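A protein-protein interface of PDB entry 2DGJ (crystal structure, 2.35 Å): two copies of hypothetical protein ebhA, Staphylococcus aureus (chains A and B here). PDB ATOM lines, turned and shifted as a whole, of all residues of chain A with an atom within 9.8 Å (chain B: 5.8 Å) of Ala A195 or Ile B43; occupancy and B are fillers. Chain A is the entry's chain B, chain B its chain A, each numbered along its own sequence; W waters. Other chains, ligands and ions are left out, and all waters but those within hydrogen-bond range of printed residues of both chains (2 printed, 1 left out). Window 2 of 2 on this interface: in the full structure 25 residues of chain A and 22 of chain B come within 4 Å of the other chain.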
ATOM      1  N   ALA A 135       6.421 -32.833 -18.251  1.00  0.00           N
ATOM      2  CA  ALA A 135       7.484 -32.254 -19.056  1.00  0.00           C
ATOM      3  C   ALA A 135       8.690 -31.848 -18.226  1.00  0.00           C
ATOM      4  O   ALA A 135       9.796 -31.755 -18.752  1.00  0.00           O
ATOM      5  CB  ALA A 135       6.961 -31.054 -19.820  1.00  0.00           C
ATOM      6  N   ASP A 138      11.861 -34.740 -15.270  1.00  0.00           N
ATOM      7  CA  ASP A 138      13.283 -35.061 -15.361  1.00  0.00           C
ATOM      8  C   ASP A 138      14.157 -33.815 -15.232  1.00  0.00           C
ATOM      9  O   ASP A 138      15.250 -33.741 -15.796  1.00  0.00           O
ATOM     10  CB  ASP A 138      13.570 -35.787 -16.682  1.00  0.00           C
ATOM     11  CG  ASP A 138      13.312 -34.921 -17.897  1.00  0.00           C
ATOM     12  OD1 ASP A 138      12.617 -33.894 -17.753  1.00  0.00           O
ATOM     13  OD2 ASP A 138      13.794 -35.272 -18.997  1.00  0.00           O
ATOM     14  N   THR A 142      18.288 -33.656 -15.809  1.00  0.00           N
ATOM     15  CA  THR A 142      18.748 -32.786 -16.887  1.00  0.00           C
ATOM     16  C   THR A 142      19.780 -31.768 -16.412  1.00  0.00           C
ATOM     17  O   THR A 142      20.827 -31.589 -17.037  1.00  0.00           O
ATOM     18  CB  THR A 142      17.560 -32.027 -17.531  1.00  0.00           C
ATOM     19  OG1 THR A 142      16.619 -32.970 -18.064  1.00  0.00           O
ATOM     20  CG2 THR A 142      18.048 -31.128 -18.653  1.00  0.00           C
ATOM     21  N   ASN A 147      25.179 -32.540 -20.978  1.00  0.00           N
ATOM     22  CA  ASN A 147      24.507 -31.952 -22.131  1.00  0.00           C
ATOM     23  C   ASN A 147      23.889 -30.616 -21.752  1.00  0.00           C
ATOM     24  O   ASN A 147      23.659 -29.770 -22.609  1.00  0.00           O
ATOM     25  CB  ASN A 147      23.428 -32.882 -22.673  1.00  0.00           C
ATOM     26  CG  ASN A 147      22.843 -32.386 -23.982  1.00  0.00           C
ATOM     27  OD1 ASN A 147      23.566 -32.167 -24.952  1.00  0.00           O
ATOM     28  ND2 ASN A 147      21.527 -32.213 -24.018  1.00  0.00           N
ATOM     29  N   TYR A 148      23.608 -30.434 -20.466  1.00  0.00           N
ATOM     30  CA  TYR A 148      23.055 -29.170 -19.991  1.00  0.00           C
ATOM     31  C   TYR A 148      24.185 -28.270 -19.493  1.00  0.00           C
ATOM     32  O   TYR A 148      24.287 -27.109 -19.888  1.00  0.00           O
ATOM     33  CB  TYR A 148      22.044 -29.378 -18.852  1.00  0.00           C
ATOM     34  CG  TYR A 148      21.765 -28.099 -18.088  1.00  0.00           C
ATOM     35  CD1 TYR A 148      22.610 -27.681 -17.061  1.00  0.00           C
ATOM     36  CD2 TYR A 148      20.709 -27.265 -18.453  1.00  0.00           C
ATOM     37  CE1 TYR A 148      22.421 -26.474 -16.426  1.00  0.00           C
ATOM     38  CE2 TYR A 148      20.509 -26.051 -17.820  1.00  0.00           C
ATOM     39  CZ  TYR A 148      21.374 -25.660 -16.812  1.00  0.00           C
ATOM     40  OH  TYR A 148      21.222 -24.439 -16.209  1.00  0.00           O
ATOM     41  N   ALA A 151      26.067 -26.769 -22.196  1.00  0.00           N
ATOM     42  CA  ALA A 151      25.228 -26.142 -23.207  1.00  0.00           C
ATOM     43  C   ALA A 151      25.478 -24.637 -23.220  1.00  0.00           C
ATOM     44  O   ALA A 151      25.864 -24.057 -22.205  1.00  0.00           O
ATOM     45  CB  ALA A 151      23.764 -26.420 -22.916  1.00  0.00           C
ATOM     46  N   LYS A 155      21.142 -21.203 -24.033  1.00  0.00           N
ATOM     47  CA  LYS A 155      20.301 -22.394 -24.076  1.00  0.00           C
ATOM     48  C   LYS A 155      19.980 -22.905 -22.677  1.00  0.00           C
ATOM     49  O   LYS A 155      18.886 -23.396 -22.426  1.00  0.00           O
ATOM     50  CB  LYS A 155      20.976 -23.491 -24.898  1.00  0.00           C
ATOM     51  CG  LYS A 155      21.258 -23.076 -26.331  1.00  0.00           C
ATOM     52  CD  LYS A 155      21.714 -24.255 -27.179  1.00  0.00           C
ATOM     53  CE  LYS A 155      22.150 -23.799 -28.562  1.00  0.00           C
ATOM     54  NZ  LYS A 155      21.085 -23.027 -29.259  1.00  0.00           N
ATOM     55  N   ALA A 158      17.345 -20.608 -21.293  1.00  0.00           N
ATOM     56  CA  ALA A 158      16.056 -20.894 -21.907  1.00  0.00           C
ATOM     57  C   ALA A 158      15.370 -22.068 -21.217  1.00  0.00           C
ATOM     58  O   ALA A 158      14.167 -22.035 -20.980  1.00  0.00           O
ATOM     59  CB  ALA A 158      16.231 -21.184 -23.401  1.00  0.00           C
ATOM     60  N   TYR A 159      16.138 -23.101 -20.891  1.00  0.00           N
ATOM     61  CA  TYR A 159      15.583 -24.276 -20.236  1.00  0.00           C
ATOM     62  C   TYR A 159      15.236 -24.000 -18.783  1.00  0.00           C
ATOM     63  O   TYR A 159      14.227 -24.488 -18.276  1.00  0.00           O
ATOM     64  CB  TYR A 159      16.564 -25.450 -20.320  1.00  0.00           C
ATOM     65  CG  TYR A 159      16.124 -26.659 -19.526  1.00  0.00           C
ATOM     66  CD1 TYR A 159      16.731 -26.980 -18.314  1.00  0.00           C
ATOM     67  CD2 TYR A 159      15.084 -27.471 -19.977  1.00  0.00           C
ATOM     68  CE1 TYR A 159      16.315 -28.081 -17.568  1.00  0.00           C
ATOM     69  CE2 TYR A 159      14.656 -28.575 -19.236  1.00  0.00           C
ATOM     70  CZ  TYR A 159      15.277 -28.872 -18.033  1.00  0.00           C
ATOM     71  OH  TYR A 159      14.850 -29.952 -17.291  1.00  0.00           O
ATOM     72  N   ALA A 162      12.139 -21.659 -18.801  1.00  0.00           N
ATOM     73  CA  ALA A 162      10.960 -22.438 -19.161  1.00  0.00           C
ATOM     74  C   ALA A 162      10.519 -23.381 -18.046  1.00  0.00           C
ATOM     75  O   ALA A 162       9.320 -23.526 -17.788  1.00  0.00           O
ATOM     76  CB  ALA A 162      11.227 -23.226 -20.438  1.00  0.00           C
ATOM     77  N   VAL A 163      11.478 -24.031 -17.393  1.00  0.00           N
ATOM     78  CA  VAL A 163      11.157 -24.945 -16.301  1.00  0.00           C
ATOM     79  C   VAL A 163      10.548 -24.188 -15.117  1.00  0.00           C
ATOM     80  O   VAL A 163       9.488 -24.558 -14.608  1.00  0.00           O
ATOM     81  CB  VAL A 163      12.413 -25.697 -15.811  1.00  0.00           C
ATOM     82  CG1 VAL A 163      12.125 -26.420 -14.503  1.00  0.00           C
ATOM     83  CG2 VAL A 163      12.860 -26.695 -16.859  1.00  0.00           C
ATOM     84  N   LEU A 187       4.390 -25.545 -22.101  1.00  0.00           N
ATOM     85  CA  LEU A 187       4.780 -26.932 -22.337  1.00  0.00           C
ATOM     86  C   LEU A 187       5.751 -27.025 -23.516  1.00  0.00           C
ATOM     87  O   LEU A 187       6.781 -27.699 -23.430  1.00  0.00           O
ATOM     88  CB  LEU A 187       3.535 -27.786 -22.606  1.00  0.00           C
ATOM     89  CG  LEU A 187       3.720 -29.222 -23.111  1.00  0.00           C
ATOM     90  CD1 LEU A 187       4.753 -29.956 -22.284  1.00  0.00           C
ATOM     91  CD2 LEU A 187       2.387 -29.937 -23.047  1.00  0.00           C
ATOM     92  N   ASN A 188       5.418 -26.345 -24.611  1.00  0.00           N
ATOM     93  CA  ASN A 188       6.273 -26.345 -25.792  1.00  0.00           C
ATOM     94  C   ASN A 188       7.640 -25.731 -25.511  1.00  0.00           C
ATOM     95  O   ASN A 188       8.645 -26.155 -26.085  1.00  0.00           O
ATOM     96  CB  ASN A 188       5.602 -25.586 -26.938  1.00  0.00           C
ATOM     97  CG  ASN A 188       4.565 -26.420 -27.654  1.00  0.00           C
ATOM     98  OD1 ASN A 188       4.874 -27.492 -28.180  1.00  0.00           O
ATOM     99  ND2 ASN A 188       3.327 -25.933 -27.686  1.00  0.00           N
ATOM    100  N   ALA A 189       7.674 -24.734 -24.630  1.00  0.00           N
ATOM    101  CA  ALA A 189       8.922 -24.064 -24.273  1.00  0.00           C
ATOM    102  C   ALA A 189       9.887 -25.031 -23.591  1.00  0.00           C
ATOM    103  O   ALA A 189      11.065 -25.089 -23.932  1.00  0.00           O
ATOM    104  CB  ALA A 189       8.640 -22.873 -23.359  1.00  0.00           C
ATOM    105  N   VAL A 190       9.382 -25.792 -22.627  1.00  0.00           N
ATOM    106  CA  VAL A 190      10.209 -26.762 -21.912  1.00  0.00           C
ATOM    107  C   VAL A 190      10.762 -27.814 -22.875  1.00  0.00           C
ATOM    108  O   VAL A 190      11.963 -28.088 -22.896  1.00  0.00           O
ATOM    109  CB  VAL A 190       9.403 -27.476 -20.804  1.00  0.00           C
ATOM    110  CG1 VAL A 190      10.206 -28.638 -20.242  1.00  0.00           C
ATOM    111  CG2 VAL A 190       9.042 -26.486 -19.694  1.00  0.00           C
ATOM    112  N   THR A 191       9.874 -28.397 -23.672  1.00  0.00           N
ATOM    113  CA  THR A 191      10.262 -29.421 -24.633  1.00  0.00           C
ATOM    114  C   THR A 191      11.323 -28.918 -25.605  1.00  0.00           C
ATOM    115  O   THR A 191      12.346 -29.568 -25.802  1.00  0.00           O
ATOM    116  CB  THR A 191       9.044 -29.914 -25.437  1.00  0.00           C
ATOM    117  OG1 THR A 191       8.070 -30.462 -24.539  1.00  0.00           O
ATOM    118  CG2 THR A 191       9.464 -30.984 -26.437  1.00  0.00           C
ATOM    119  N   ARG A 192      11.079 -27.760 -26.209  1.00  0.00           N
ATOM    120  CA  ARG A 192      12.027 -27.193 -27.161  1.00  0.00           C
ATOM    121  C   ARG A 192      13.349 -26.799 -26.517  1.00  0.00           C
ATOM    122  O   ARG A 192      14.419 -27.010 -27.096  1.00  0.00           O
ATOM    123  CB  ARG A 192      11.407 -25.980 -27.849  1.00  0.00           C
ATOM    124  CG  ARG A 192      10.377 -26.349 -28.902  1.00  0.00           C
ATOM    125  CD  ARG A 192       9.585 -25.141 -29.374  1.00  0.00           C
ATOM    126  NE  ARG A 192       8.563 -25.516 -30.349  1.00  0.00           N
ATOM    127  CZ  ARG A 192       7.484 -24.788 -30.623  1.00  0.00           C
ATOM    128  NH1 ARG A 192       7.274 -23.637 -30.000  1.00  0.00           N
ATOM    129  NH2 ARG A 192       6.605 -25.219 -31.518  1.00  0.00           N
ATOM    130  N   ALA A 193      13.273 -26.237 -25.313  1.00  0.00           N
ATOM    131  CA  ALA A 193      14.469 -25.815 -24.603  1.00  0.00           C
ATOM    132  C   ALA A 193      15.325 -27.000 -24.186  1.00  0.00           C
ATOM    133  O   ALA A 193      16.548 -26.955 -24.306  1.00  0.00           O
ATOM    134  CB  ALA A 193      14.092 -24.983 -23.371  1.00  0.00           C
ATOM    135  N   LYS A 194      14.688 -28.064 -23.703  1.00  0.00           N
ATOM    136  CA  LYS A 194      15.431 -29.239 -23.269  1.00  0.00           C
ATOM    137  C   LYS A 194      16.086 -29.927 -24.462  1.00  0.00           C
ATOM    138  O   LYS A 194      17.251 -30.318 -24.402  1.00  0.00           O
ATOM    139  CB  LYS A 194      14.508 -30.223 -22.545  1.00  0.00           C
ATOM    140  CG  LYS A 194      15.263 -31.239 -21.702  1.00  0.00           C
ATOM    141  CD  LYS A 194      14.339 -32.218 -20.995  1.00  0.00           C
ATOM    142  CE  LYS A 194      13.720 -33.217 -21.960  1.00  0.00           C
ATOM    143  NZ  LYS A 194      12.810 -34.170 -21.259  1.00  0.00           N
ATOM    144  N   ALA A 195      15.338 -30.050 -25.554  1.00  0.00           N
ATOM    145  CA  ALA A 195      15.848 -30.681 -26.766  1.00  0.00           C
ATOM    146  C   ALA A 195      16.919 -29.811 -27.411  1.00  0.00           C
ATOM    147  O   ALA A 195      17.745 -30.305 -28.184  1.00  0.00           O
ATOM    148  CB  ALA A 195      14.705 -30.924 -27.756  1.00  0.00           C
ATOM    149  N   ALA A 196      16.906 -28.521 -27.087  1.00  0.00           N
ATOM    150  CA  ALA A 196      17.868 -27.577 -27.646  1.00  0.00           C
ATOM    151  C   ALA A 196      19.230 -27.635 -26.960  1.00  0.00           C
ATOM    152  O   ALA A 196      20.233 -27.226 -27.539  1.00  0.00           O
ATOM    153  CB  ALA A 196      17.312 -26.164 -27.578  1.00  0.00           C
ATOM    154  N   LEU A 197      19.264 -28.125 -25.724  1.00  0.00           N
ATOM    155  CA  LEU A 197      20.519 -28.240 -24.986  1.00  0.00           C
ATOM    156  C   LEU A 197      21.573 -28.874 -25.893  1.00  0.00           C
ATOM    157  O   LEU A 197      21.386 -29.983 -26.395  1.00  0.00           O
ATOM    158  CB  LEU A 197      20.309 -29.086 -23.728  1.00  0.00           C
ATOM    159  CG  LEU A 197      20.042 -28.336 -22.417  1.00  0.00           C
ATOM    160  CD1 LEU A 197      19.393 -26.986 -22.682  1.00  0.00           C
ATOM    161  CD2 LEU A 197      19.167 -29.194 -21.521  1.00  0.00           C
ATOM    162  N   ASN A 198      22.679 -28.166 -26.095  1.00  0.00           N
ATOM    163  CA  ASN A 198      23.741 -28.637 -26.978  1.00  0.00           C
ATOM    164  C   ASN A 198      25.097 -28.863 -26.301  1.00  0.00           C
ATOM    165  O   ASN A 198      26.141 -28.713 -26.932  1.00  0.00           O
ATOM    166  CB  ASN A 198      23.905 -27.642 -28.130  1.00  0.00           C
ATOM    167  CG  ASN A 198      24.426 -26.296 -27.662  1.00  0.00           C
ATOM    168  OD1 ASN A 198      24.069 -25.821 -26.582  1.00  0.00           O
ATOM    169  ND2 ASN A 198      25.269 -25.670 -28.475  1.00  0.00           N
ATOM    170  N   GLY A 199      25.080 -29.227 -25.022  1.00  0.00           N
ATOM    171  CA  GLY A 199      26.325 -29.474 -24.312  1.00  0.00           C
ATOM    172  C   GLY A 199      27.107 -30.578 -24.995  1.00  0.00           C
ATOM    173  O   GLY A 199      28.340 -30.561 -25.036  1.00  0.00           O
ATOM    174  N   ALA A 200      26.379 -31.541 -25.548  1.00  0.00           N
ATOM    175  CA  ALA A 200      26.987 -32.664 -26.246  1.00  0.00           C
ATOM    176  C   ALA A 200      27.745 -32.180 -27.476  1.00  0.00           C
ATOM    177  O   ALA A 200      28.864 -32.621 -27.744  1.00  0.00           O
ATOM    178  CB  ALA A 200      25.909 -33.651 -26.648  1.00  0.00           C
ATOM    179  N   GLU A 201      27.124 -31.273 -28.221  1.00  0.00           N
ATOM    180  CA  GLU A 201      27.729 -30.716 -29.422  1.00  0.00           C
ATOM    181  C   GLU A 201      28.933 -29.847 -29.091  1.00  0.00           C
ATOM    182  O   GLU A 201      29.967 -29.946 -29.754  1.00  0.00           O
ATOM    183  CB  GLU A 201      26.696 -29.897 -30.197  1.00  0.00           C
ATOM    184  CG  GLU A 201      25.859 -30.702 -31.181  1.00  0.00           C
ATOM    185  CD  GLU A 201      25.334 -32.009 -30.601  1.00  0.00           C
ATOM    186  OE1 GLU A 201      26.150 -32.917 -30.327  1.00  0.00           O
ATOM    187  OE2 GLU A 201      24.102 -32.131 -30.425  1.00  0.00           O
ATOM    188  N   LEU B   6      14.248 -39.717 -38.873  1.00  0.00           N
ATOM    189  CA  LEU B   6      13.818 -38.664 -37.959  1.00  0.00           C
ATOM    190  C   LEU B   6      13.177 -37.532 -38.757  1.00  0.00           C
ATOM    191  O   LEU B   6      12.140 -36.988 -38.362  1.00  0.00           O
ATOM    192  CB  LEU B   6      15.013 -38.131 -37.166  1.00  0.00           C
ATOM    193  CG  LEU B   6      14.674 -37.087 -36.098  1.00  0.00           C
ATOM    194  CD1 LEU B   6      13.755 -37.694 -35.040  1.00  0.00           C
ATOM    195  CD2 LEU B   6      15.956 -36.582 -35.468  1.00  0.00           C
ATOM    196  N   ALA B  38       8.093 -31.883 -31.803  1.00  0.00           N
ATOM    197  CA  ALA B  38       8.747 -30.624 -31.471  1.00  0.00           C
ATOM    198  C   ALA B  38      10.162 -30.907 -30.990  1.00  0.00           C
ATOM    199  O   ALA B  38      11.112 -30.216 -31.365  1.00  0.00           O
ATOM    200  CB  ALA B  38       7.957 -29.891 -30.396  1.00  0.00           C
ATOM    201  N   ALA B  39      10.298 -31.936 -30.164  1.00  0.00           N
ATOM    202  CA  ALA B  39      11.596 -32.324 -29.640  1.00  0.00           C
ATOM    203  C   ALA B  39      12.518 -32.749 -30.790  1.00  0.00           C
ATOM    204  O   ALA B  39      13.692 -32.374 -30.837  1.00  0.00           O
ATOM    205  CB  ALA B  39      11.430 -33.464 -28.658  1.00  0.00           C
ATOM    206  N   ALA B  40      11.969 -33.538 -31.712  1.00  0.00           N
ATOM    207  CA  ALA B  40      12.720 -34.032 -32.861  1.00  0.00           C
ATOM    208  C   ALA B  40      13.281 -32.878 -33.685  1.00  0.00           C
ATOM    209  O   ALA B  40      14.462 -32.864 -34.020  1.00  0.00           O
ATOM    210  CB  ALA B  40      11.826 -34.918 -33.738  1.00  0.00           C
ATOM    211  N   LYS B  41      12.430 -31.906 -34.000  1.00  0.00           N
ATOM    212  CA  LYS B  41      12.863 -30.753 -34.783  1.00  0.00           C
ATOM    213  C   LYS B  41      14.079 -30.103 -34.145  1.00  0.00           C
ATOM    214  O   LYS B  41      15.086 -29.854 -34.804  1.00  0.00           O
ATOM    215  CB  LYS B  41      11.741 -29.709 -34.889  1.00  0.00           C
ATOM    216  CG  LYS B  41      10.550 -30.126 -35.730  1.00  0.00           C
ATOM    217  CD  LYS B  41       9.500 -29.019 -35.746  1.00  0.00           C
ATOM    218  CE  LYS B  41       8.234 -29.438 -36.479  1.00  0.00           C
ATOM    219  NZ  LYS B  41       7.168 -28.408 -36.332  1.00  0.00           N
ATOM    220  N   ALA B  42      13.974 -29.816 -32.853  1.00  0.00           N
ATOM    221  CA  ALA B  42      15.050 -29.179 -32.113  1.00  0.00           C
ATOM    222  C   ALA B  42      16.325 -30.017 -32.164  1.00  0.00           C
ATOM    223  O   ALA B  42      17.408 -29.503 -32.444  1.00  0.00           O
ATOM    224  CB  ALA B  42      14.624 -28.960 -30.669  1.00  0.00           C
ATOM    225  N   ILE B  43      16.184 -31.311 -31.897  1.00  0.00           N
ATOM    226  CA  ILE B  43      17.320 -32.222 -31.913  1.00  0.00           C
ATOM    227  C   ILE B  43      17.934 -32.302 -33.306  1.00  0.00           C
ATOM    228  O   ILE B  43      19.158 -32.289 -33.449  1.00  0.00           O
ATOM    229  CB  ILE B  43      16.901 -33.635 -31.462  1.00  0.00           C
ATOM    230  CG1 ILE B  43      16.552 -33.617 -29.972  1.00  0.00           C
ATOM    231  CG2 ILE B  43      18.024 -34.631 -31.749  1.00  0.00           C
ATOM    232  CD1 ILE B  43      16.016 -34.933 -29.438  1.00  0.00           C
ATOM    233  N   LEU B  44      17.093 -32.378 -34.331  1.00  0.00           N
ATOM    234  CA  LEU B  44      17.583 -32.462 -35.700  1.00  0.00           C
ATOM    235  C   LEU B  44      18.334 -31.182 -36.067  1.00  0.00           C
ATOM    236  O   LEU B  44      19.317 -31.216 -36.799  1.00  0.00           O
ATOM    237  CB  LEU B  44      16.420 -32.670 -36.668  1.00  0.00           C
ATOM    238  CG  LEU B  44      16.799 -33.171 -38.063  1.00  0.00           C
ATOM    239  CD1 LEU B  44      17.408 -34.552 -37.940  1.00  0.00           C
ATOM    240  CD2 LEU B  44      15.574 -33.228 -38.950  1.00  0.00           C
ATOM    241  N   ASN B  45      17.858 -30.056 -35.544  1.00  0.00           N
ATOM    242  CA  ASN B  45      18.479 -28.759 -35.807  1.00  0.00           C
ATOM    243  C   ASN B  45      19.903 -28.710 -35.252  1.00  0.00           C
ATOM    244  O   ASN B  45      20.827 -28.258 -35.929  1.00  0.00           O
ATOM    245  CB  ASN B  45      17.631 -27.637 -35.188  1.00  0.00           C
ATOM    246  CG  ASN B  45      18.220 -26.265 -35.430  1.00  0.00           C
ATOM    247  OD1 ASN B  45      18.641 -25.946 -36.544  1.00  0.00           O
ATOM    248  ND2 ASN B  45      18.248 -25.437 -34.389  1.00  0.00           N
ATOM    249  N   LYS B  46      20.076 -29.180 -34.020  1.00  0.00           N
ATOM    250  CA  LYS B  46      21.383 -29.194 -33.372  1.00  0.00           C
ATOM    251  C   LYS B  46      22.474 -29.793 -34.256  1.00  0.00           C
ATOM    252  O   LYS B  46      23.596 -29.292 -34.288  1.00  0.00           O
ATOM    253  CB  LYS B  46      21.302 -29.967 -32.054  1.00  0.00           C
ATOM    254  CG  LYS B  46      20.807 -29.138 -30.887  1.00  0.00           C
ATOM    255  CD  LYS B  46      20.198 -30.017 -29.798  1.00  0.00           C
ATOM    256  CE  LYS B  46      21.127 -31.143 -29.361  1.00  0.00           C
ATOM    257  NZ  LYS B  46      20.466 -32.039 -28.358  1.00  0.00           N
ATOM    258  N   GLN B  47      22.146 -30.871 -34.961  1.00  0.00           N
ATOM    259  CA  GLN B  47      23.112 -31.515 -35.844  1.00  0.00           C
ATOM    260  C   GLN B  47      23.305 -30.735 -37.138  1.00  0.00           C
ATOM    261  O   GLN B  47      22.343 -30.404 -37.830  1.00  0.00           O
ATOM    262  CB  GLN B  47      22.679 -32.951 -36.168  1.00  0.00           C
ATOM    263  CG  GLN B  47      23.160 -33.988 -35.162  1.00  0.00           C
ATOM    264  CD  GLN B  47      22.217 -34.159 -33.988  1.00  0.00           C
ATOM    265  OE1 GLN B  47      21.537 -33.222 -33.579  1.00  0.00           O
ATOM    266  NE2 GLN B  47      22.189 -35.362 -33.427  1.00  0.00           N
ATOM    267  N   ALA B  56      21.232 -39.585 -29.861  1.00  0.00           N
ATOM    268  CA  ALA B  56      20.248 -38.566 -29.505  1.00  0.00           C
ATOM    269  C   ALA B  56      19.205 -38.517 -30.617  1.00  0.00           C
ATOM    270  O   ALA B  56      18.016 -38.311 -30.371  1.00  0.00           O
ATOM    271  CB  ALA B  56      20.924 -37.201 -29.358  1.00  0.00           C
ATOM    272  N   VAL B  57      19.666 -38.715 -31.847  1.00  0.00           N
ATOM    273  CA  VAL B  57      18.788 -38.709 -33.006  1.00  0.00           C
ATOM    274  C   VAL B  57      17.878 -39.932 -32.985  1.00  0.00           C
ATOM    275  O   VAL B  57      16.721 -39.855 -33.394  1.00  0.00           O
ATOM    276  CB  VAL B  57      19.597 -38.732 -34.325  1.00  0.00           C
ATOM    277  CG1 VAL B  57      18.657 -38.777 -35.518  1.00  0.00           C
ATOM    278  CG2 VAL B  57      20.480 -37.512 -34.411  1.00  0.00           C
ATOM    279  N   ALA B  60      15.211 -39.732 -30.245  1.00  0.00           N
ATOM    280  CA  ALA B  60      14.204 -38.792 -30.720  1.00  0.00           C
ATOM    281  C   ALA B  60      13.292 -39.505 -31.709  1.00  0.00           C
ATOM    282  O   ALA B  60      12.073 -39.349 -31.683  1.00  0.00           O
ATOM    283  CB  ALA B  60      14.883 -37.605 -31.386  1.00  0.00           C
HETATM  284  O   HOH W   1       6.759 -27.335 -33.237  1.00  0.00           O
HETATM  285  O   HOH W   2      11.004 -27.491 -31.670  1.00  0.00           O
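NZ of Lys B46 lies close to O of Ala A195, 3.2 Å away.
The side-chain amino group (NZ) of Lys B46 sits at hydrogen-bond distance from the backbone carbonyl oxygen (O) of Leu A197 (3.0 Å).
ND2 of Asn A147 is in hydrogen-bond range of O of Leu A197 (3.3 Å).
OG1 of Thr A191 sits at hydrogen-bond distance from O of Leu A187.
The backbone carbonyl oxygen of Ile B43 sits close to the side-chain amide oxygen of Gln B47.
CG2 of Thr A191 touches CB of Ala B39, 3.9 Å away.
Ala B39 touches Ala A195.
Ala A195 touches Ala B42 (CB to CB, 3.5 Å).
Ala A195 touches Ile B43.
Ala A196 touches Lys B46.
OE2 of Glu A201 touches CE of Lys B46, 3.3 Å away.
Of the printed residues of chain B, Thr A191 touches Ala B39 (3.9 Å).
Ala A195 touches four residues of chain B.
Of the printed residues of chain B, Ala A196 touches Lys B46 (3.6 Å).
Of the printed residues of chain B, Leu A197 touches Lys B46.
Of the printed residues of chain B, Glu A201 touches Lys B46.
Ala B39 touches just these residues of chain A: Thr A191 and Ala A195.
Ala B40 touches none of the printed residues of chain A.
Ala B42 touches just one residue of chain A: Ala A195.
Of chain A, only Ala A195 (3.9 Å) comes within 4 Å of Ile B43.
Of chain A, only Ala A195, Ala A196, Leu A197 and Glu A201 come within 4 Å of Lys B46.
The nearest residue of chain B that does not touch Ala A195 is Ala B38 (5.1 Å).
Hydrophobic or aromatic side chains of chain A that line the printed part of chain B: Ala A195.
Of the 14 printed residues of chain B, 4 touch a printed residue of chain A.
No position is printed for both chains.
Of the 8 pairs that touch across the chains among the printed residues, none has its exchanged pair printed and touching as well.
Water W1 bridges the guanidinium group of Arg A192 (2.7 Å) and the side-chain amino group of Lys B41 (3.3 Å).
Water W2 bridges the backbone carbonyl oxygen of Ala B38 (2.7 Å) and the guanidinium group of Arg A192 (3.4 Å).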
